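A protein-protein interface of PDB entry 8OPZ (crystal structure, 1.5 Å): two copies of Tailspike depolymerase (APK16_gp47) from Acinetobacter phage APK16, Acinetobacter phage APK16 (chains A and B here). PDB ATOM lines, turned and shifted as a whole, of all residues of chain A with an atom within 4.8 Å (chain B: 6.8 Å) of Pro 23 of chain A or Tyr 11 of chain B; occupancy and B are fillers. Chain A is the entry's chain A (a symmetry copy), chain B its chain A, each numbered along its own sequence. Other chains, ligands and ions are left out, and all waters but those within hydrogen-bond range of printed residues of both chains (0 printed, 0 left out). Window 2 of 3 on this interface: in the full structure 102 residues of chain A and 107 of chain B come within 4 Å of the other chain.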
ATOM      1  N   ILE A  20     -15.562  24.639  -8.565  1.00  0.00           N
ATOM      2  CA  ILE A  20     -16.047  23.528  -7.741  1.00  0.00           C
ATOM      3  C   ILE A  20     -14.882  22.788  -7.066  1.00  0.00           C
ATOM      4  O   ILE A  20     -13.829  22.582  -7.674  1.00  0.00           O
ATOM      5  CB  ILE A  20     -17.042  22.628  -8.542  1.00  0.00           C
ATOM      6  CG1 ILE A  20     -18.431  23.287  -8.609  1.00  0.00           C
ATOM      7  CG2 ILE A  20     -17.146  21.170  -8.060  1.00  0.00           C
ATOM      8  CD1 ILE A  20     -19.348  22.828  -9.748  1.00  0.00           C
ATOM      9  N   VAL A  21     -15.154  22.359  -5.818  1.00  0.00           N
ATOM     10  CA  VAL A  21     -14.438  21.359  -5.029  1.00  0.00           C
ATOM     11  C   VAL A  21     -15.153  20.012  -5.170  1.00  0.00           C
ATOM     12  O   VAL A  21     -16.363  19.904  -4.911  1.00  0.00           O
ATOM     13  CB  VAL A  21     -14.257  21.813  -3.560  1.00  0.00           C
ATOM     14  CG1 VAL A  21     -14.015  20.687  -2.551  1.00  0.00           C
ATOM     15  CG2 VAL A  21     -13.134  22.837  -3.471  1.00  0.00           C
ATOM     16  N   TYR A  22     -14.362  19.017  -5.602  1.00  0.00           N
ATOM     17  CA  TYR A  22     -14.822  17.665  -5.854  1.00  0.00           C
ATOM     18  C   TYR A  22     -14.595  16.847  -4.597  1.00  0.00           C
ATOM     19  O   TYR A  22     -13.470  16.867  -4.083  1.00  0.00           O
ATOM     20  CB  TYR A  22     -14.206  17.078  -7.125  1.00  0.00           C
ATOM     21  CG  TYR A  22     -14.644  17.834  -8.351  1.00  0.00           C
ATOM     22  CD1 TYR A  22     -13.894  18.917  -8.832  1.00  0.00           C
ATOM     23  CD2 TYR A  22     -15.850  17.526  -8.992  1.00  0.00           C
ATOM     24  CE1 TYR A  22     -14.293  19.609  -9.978  1.00  0.00           C
ATOM     25  CE2 TYR A  22     -16.281  18.244 -10.110  1.00  0.00           C
ATOM     26  CZ  TYR A  22     -15.492  19.272 -10.609  1.00  0.00           C
ATOM     27  OH  TYR A  22     -15.908  19.972 -11.700  1.00  0.00           O
ATOM     28  N   PRO A  23     -15.627  16.141  -4.043  1.00  0.00           N
ATOM     29  CA  PRO A  23     -15.414  15.171  -2.959  1.00  0.00           C
ATOM     30  C   PRO A  23     -14.793  13.897  -3.538  1.00  0.00           C
ATOM     31  O   PRO A  23     -14.792  13.668  -4.758  1.00  0.00           O
ATOM     32  CB  PRO A  23     -16.831  14.942  -2.411  1.00  0.00           C
ATOM     33  CG  PRO A  23     -17.750  15.182  -3.591  1.00  0.00           C
ATOM     34  CD  PRO A  23     -17.019  16.127  -4.507  1.00  0.00           C
ATOM     35  N   LYS A  24     -14.348  13.015  -2.641  1.00  0.00           N
ATOM     36  CA  LYS A  24     -13.782  11.713  -2.947  1.00  0.00           C
ATOM     37  C   LYS A  24     -14.866  10.882  -3.647  1.00  0.00           C
ATOM     38  O   LYS A  24     -16.030  10.964  -3.235  1.00  0.00           O
ATOM     39  CB  LYS A  24     -13.388  11.090  -1.609  1.00  0.00           C
ATOM     40  N   ASN A  25     -14.494  10.107  -4.696  1.00  0.00           N
ATOM     41  CA  ASN A  25     -15.417   9.277  -5.490  1.00  0.00           C
ATOM     42  C   ASN A  25     -16.198  10.033  -6.580  1.00  0.00           C
ATOM     43  O   ASN A  25     -16.924   9.360  -7.325  1.00  0.00           O
ATOM     44  CB  ASN A  25     -16.140   8.231  -4.624  1.00  0.00           C
ATOM     45  CG  ASN A  25     -15.228   7.559  -3.619  1.00  0.00           C
ATOM     46  OD1 ASN A  25     -14.133   7.062  -3.936  1.00  0.00           O
ATOM     47  ND2 ASN A  25     -15.722   7.455  -2.401  1.00  0.00           N
ATOM     48  N   ALA A  26     -16.094  11.396  -6.651  1.00  0.00           N
ATOM     49  CA  ALA A  26     -16.760  12.226  -7.655  1.00  0.00           C
ATOM     50  C   ALA A  26     -16.137  11.905  -9.002  1.00  0.00           C
ATOM     51  O   ALA A  26     -14.901  11.870  -9.178  1.00  0.00           O
ATOM     52  CB  ALA A  26     -16.684  13.697  -7.379  1.00  0.00           C
ATOM     53  N   ARG A  27     -17.068  11.657  -9.925  1.00  0.00           N
ATOM     54  CA  ARG A  27     -16.837  11.376 -11.326  1.00  0.00           C
ATOM     55  C   ARG A  27     -17.363  12.504 -12.222  1.00  0.00           C
ATOM     56  O   ARG A  27     -18.543  12.883 -12.245  1.00  0.00           O
ATOM     57  CB  ARG A  27     -17.522  10.074 -11.740  1.00  0.00           C
ATOM     58  CG  ARG A  27     -16.763   8.825 -11.367  1.00  0.00           C
ATOM     59  CD  ARG A  27     -17.555   7.561 -11.680  1.00  0.00           C
ATOM     60  NE  ARG A  27     -16.931   6.496 -10.877  1.00  0.00           N
ATOM     61  CZ  ARG A  27     -16.531   5.282 -11.245  1.00  0.00           C
ATOM     62  NH1 ARG A  27     -16.694   4.832 -12.476  1.00  0.00           N
ATOM     63  NH2 ARG A  27     -15.970   4.504 -10.344  1.00  0.00           N
ATOM     64  N   ILE A  28     -16.473  12.816 -13.153  1.00  0.00           N
ATOM     65  CA  ILE A  28     -16.683  13.803 -14.204  1.00  0.00           C
ATOM     66  C   ILE A  28     -16.051  13.235 -15.473  1.00  0.00           C
ATOM     67  O   ILE A  28     -15.390  12.210 -15.422  1.00  0.00           O
ATOM     68  CB  ILE A  28     -16.183  15.232 -13.807  1.00  0.00           C
ATOM     69  CG1 ILE A  28     -14.704  15.298 -13.401  1.00  0.00           C
ATOM     70  CG2 ILE A  28     -17.096  15.851 -12.764  1.00  0.00           C
ATOM     71  CD1 ILE A  28     -14.093  16.662 -13.490  1.00  0.00           C
ATOM     72  N   SER A  38     -12.228  11.361  -8.543  1.00  0.00           N
ATOM     73  CA  SER A  38     -11.378  11.882  -7.490  1.00  0.00           C
ATOM     74  C   SER A  38     -11.083  10.845  -6.399  1.00  0.00           C
ATOM     75  O   SER A  38     -11.979  10.305  -5.730  1.00  0.00           O
ATOM     76  CB  SER A  38     -11.794  13.209  -6.963  1.00  0.00           C
ATOM     77  OG  SER A  38     -10.713  13.710  -6.165  1.00  0.00           O
ATOM     78  N   VAL A  40      -9.261  12.260  -3.887  1.00  0.00           N
ATOM     79  CA  VAL A  40      -9.236  13.225  -2.775  1.00  0.00           C
ATOM     80  C   VAL A  40     -10.573  13.968  -2.593  1.00  0.00           C
ATOM     81  O   VAL A  40     -11.310  14.157  -3.572  1.00  0.00           O
ATOM     82  CB  VAL A  40      -8.003  14.161  -2.763  1.00  0.00           C
ATOM     83  CG1 VAL A  40      -6.678  13.423  -2.587  1.00  0.00           C
ATOM     84  CG2 VAL A  40      -7.929  15.133  -3.923  1.00  0.00           C
ATOM     85  N   ASP A  41     -10.864  14.402  -1.329  1.00  0.00           N
ATOM     86  CA  ASP A  41     -12.014  15.168  -0.819  1.00  0.00           C
ATOM     87  C   ASP A  41     -11.961  16.679  -1.094  1.00  0.00           C
ATOM     88  O   ASP A  41     -13.001  17.368  -1.161  1.00  0.00           O
ATOM     89  CB  ASP A  41     -12.159  14.960   0.696  1.00  0.00           C
ATOM     90  CG  ASP A  41     -12.910  13.691   1.085  1.00  0.00           C
ATOM     91  OD1 ASP A  41     -14.049  13.522   0.611  1.00  0.00           O
ATOM     92  OD2 ASP A  41     -12.325  12.858   1.836  1.00  0.00           O
ATOM     93  N   GLN B  10     -23.496  18.908 -11.379  1.00  0.00           N
ATOM     94  CA  GLN B  10     -22.136  18.984 -10.677  1.00  0.00           C
ATOM     95  C   GLN B  10     -21.182  17.820 -11.067  1.00  0.00           C
ATOM     96  O   GLN B  10     -20.169  17.979 -11.773  1.00  0.00           O
ATOM     97  CB  GLN B  10     -22.399  19.229  -9.176  1.00  0.00           C
ATOM     98  N   TYR B  11     -21.476  16.617 -10.564  1.00  0.00           N
ATOM     99  CA  TYR B  11     -20.608  15.445 -10.674  1.00  0.00           C
ATOM    100  C   TYR B  11     -21.510  14.231 -10.450  1.00  0.00           C
ATOM    101  O   TYR B  11     -22.642  14.408  -9.969  1.00  0.00           O
ATOM    102  CB  TYR B  11     -19.434  15.535  -9.680  1.00  0.00           C
ATOM    103  CG  TYR B  11     -19.754  15.889  -8.253  1.00  0.00           C
ATOM    104  CD1 TYR B  11     -20.154  14.872  -7.351  1.00  0.00           C
ATOM    105  CD2 TYR B  11     -19.706  17.207  -7.781  1.00  0.00           C
ATOM    106  CE1 TYR B  11     -20.563  15.170  -6.052  1.00  0.00           C
ATOM    107  CE2 TYR B  11     -20.025  17.505  -6.457  1.00  0.00           C
ATOM    108  CZ  TYR B  11     -20.441  16.480  -5.601  1.00  0.00           C
ATOM    109  OH  TYR B  11     -20.713  16.755  -4.298  1.00  0.00           O
ATOM    110  N   TYR B  12     -20.937  13.030 -10.667  1.00  0.00           N
ATOM    111  CA  TYR B  12     -21.634  11.745 -10.592  1.00  0.00           C
ATOM    112  C   TYR B  12     -21.072  11.052  -9.362  1.00  0.00           C
ATOM    113  O   TYR B  12     -19.865  10.843  -9.299  1.00  0.00           O
ATOM    114  CB  TYR B  12     -21.670  10.995 -11.946  1.00  0.00           C
ATOM    115  CG  TYR B  12     -22.344  11.811 -13.030  1.00  0.00           C
ATOM    116  CD1 TYR B  12     -23.704  12.130 -12.927  1.00  0.00           C
ATOM    117  CD2 TYR B  12     -21.607  12.355 -14.083  1.00  0.00           C
ATOM    118  CE1 TYR B  12     -24.327  12.941 -13.875  1.00  0.00           C
ATOM    119  CE2 TYR B  12     -22.233  13.139 -15.058  1.00  0.00           C
ATOM    120  CZ  TYR B  12     -23.593  13.431 -14.953  1.00  0.00           C
ATOM    121  OH  TYR B  12     -24.229  14.206 -15.889  1.00  0.00           O
ATOM    122  N   LEU B  13     -21.994  10.795  -8.417  1.00  0.00           N
ATOM    123  CA  LEU B  13     -21.851  10.276  -7.057  1.00  0.00           C
ATOM    124  C   LEU B  13     -23.213  10.134  -6.381  1.00  0.00           C
ATOM    125  O   LEU B  13     -23.887  11.122  -6.102  1.00  0.00           O
ATOM    126  CB  LEU B  13     -20.866  11.106  -6.209  1.00  0.00           C
ATOM    127  CG  LEU B  13     -20.486  10.517  -4.834  1.00  0.00           C
ATOM    128  CD1 LEU B  13     -19.693   9.211  -4.936  1.00  0.00           C
ATOM    129  CD2 LEU B  13     -19.716  11.542  -4.020  1.00  0.00           C
ATOM    130  N   TYR B  15     -24.374   7.292  -3.110  1.00  0.00           N
ATOM    131  CA  TYR B  15     -24.295   6.130  -2.231  1.00  0.00           C
ATOM    132  C   TYR B  15     -25.594   5.343  -2.109  1.00  0.00           C
ATOM    133  O   TYR B  15     -26.668   5.809  -2.530  1.00  0.00           O
ATOM    134  CB  TYR B  15     -23.548   6.459  -0.939  1.00  0.00           C
ATOM    135  CG  TYR B  15     -22.147   6.992  -1.152  1.00  0.00           C
ATOM    136  CD1 TYR B  15     -21.169   6.297  -1.875  1.00  0.00           C
ATOM    137  CD2 TYR B  15     -21.815   8.275  -0.670  1.00  0.00           C
ATOM    138  CE1 TYR B  15     -19.889   6.815  -2.062  1.00  0.00           C
ATOM    139  CE2 TYR B  15     -20.524   8.792  -0.808  1.00  0.00           C
ATOM    140  CZ  TYR B  15     -19.566   8.052  -1.496  1.00  0.00           C
ATOM    141  OH  TYR B  15     -18.335   8.588  -1.645  1.00  0.00           O
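The side-chain hydroxyl of Tyr 15 of chain B lies within hydrogen-bond range of the side-chain amide nitrogen of Asn 25 of chain A, 2.9 Å away. N of Tyr 12 of chain B is in hydrogen-bond range of O of Arg 27 of chain A, at 2.9 Å.
The side-chain carboxylate (OD1) of Asp 41 of chain A is in hydrogen-bond range of the backbone NH (N) of Lys 24 of chain A (3.3 Å). N of Lys 24 of chain A sits at hydrogen-bond distance from O of Val 40 of chain A (3.4 Å). The backbone carbonyl oxygen (O) of Ala 26 of chain A lies within hydrogen-bond range of the backbone NH (N) of Ser 38 of chain A. The backbone NH of Asn 25 of chain A is in hydrogen-bond range of the backbone carbonyl oxygen of Ser 38 of chain A (2.7 Å).
Of chain B, only Tyr 11 comes within 4 Å of Pro 23 of chain A. Of the printed residues of chain B, Ala 26 of chain A touches Tyr 11 and Tyr 12. Printed residues of chain B within 4 Å of Arg 27 of chain A: Tyr 11 (3.6 Å) and Tyr 12 (2.9 Å). Of the printed residues of chain B, Ile 28 of chain A touches Gln 10 and Tyr 11. Val 40 of chain A touches none of the printed residues of chain B. Printed residues of chain A within 4 Å of Gln 10 of chain B: Ile 28. Tyr 11 of chain B touches four residues of chain A. Of the printed residues of chain A, Tyr 15 of chain B touches Lys 24 and Asn 25. The nearest residue of chain B that does not touch Pro 23 of chain A is Leu 13 of chain B (4.2 Å). The nearest residue of chain A that does not touch Tyr 11 of chain B is Tyr 22 of chain A (4.1 Å).
Among the printed residues, merely in contact across the chains: Pro 23 of chain A with Tyr 11 of chain B, Lys 24 of chain A with Leu 13 of chain B, Lys 24 of chain A with Tyr 15 of chain B, Asn 25 of chain A with Tyr 12 of chain B, Asn 25 of chain A with Leu 13 of chain B, Ala 26 of chain A with Tyr 11 of chain B, Ala 26 of chain A with Tyr 12 of chain B, Arg 27 of chain A with Tyr 11 of chain B, Ile 28 of chain A with Gln 10 of chain B and Ile 28 of chain A with Tyr 11 of chain B.
Hydrophobic or aromatic side chains of chain A that line the printed part of chain B: Pro 23, Ala 26 and Ile 28. Of the 5 printed residues of chain B, 5 touch a printed residue of chain A. Printed residues of chain B that touch a printed residue of chain A: Gln 10, Tyr 11, Tyr 12, Leu 13 and Tyr 15. Hydrophobic or aromatic side chains of chain B that line the printed part of chain A: Tyr 11, Tyr 12, Leu 13 and Tyr 15. Among the printed residues, 12 pairs touch across the chains. Among the printed residues, no Asp or Glu carboxylate lies within 4 Å of a Lys or Arg side-chain nitrogen of the other chain.
No position is printed for both chains.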
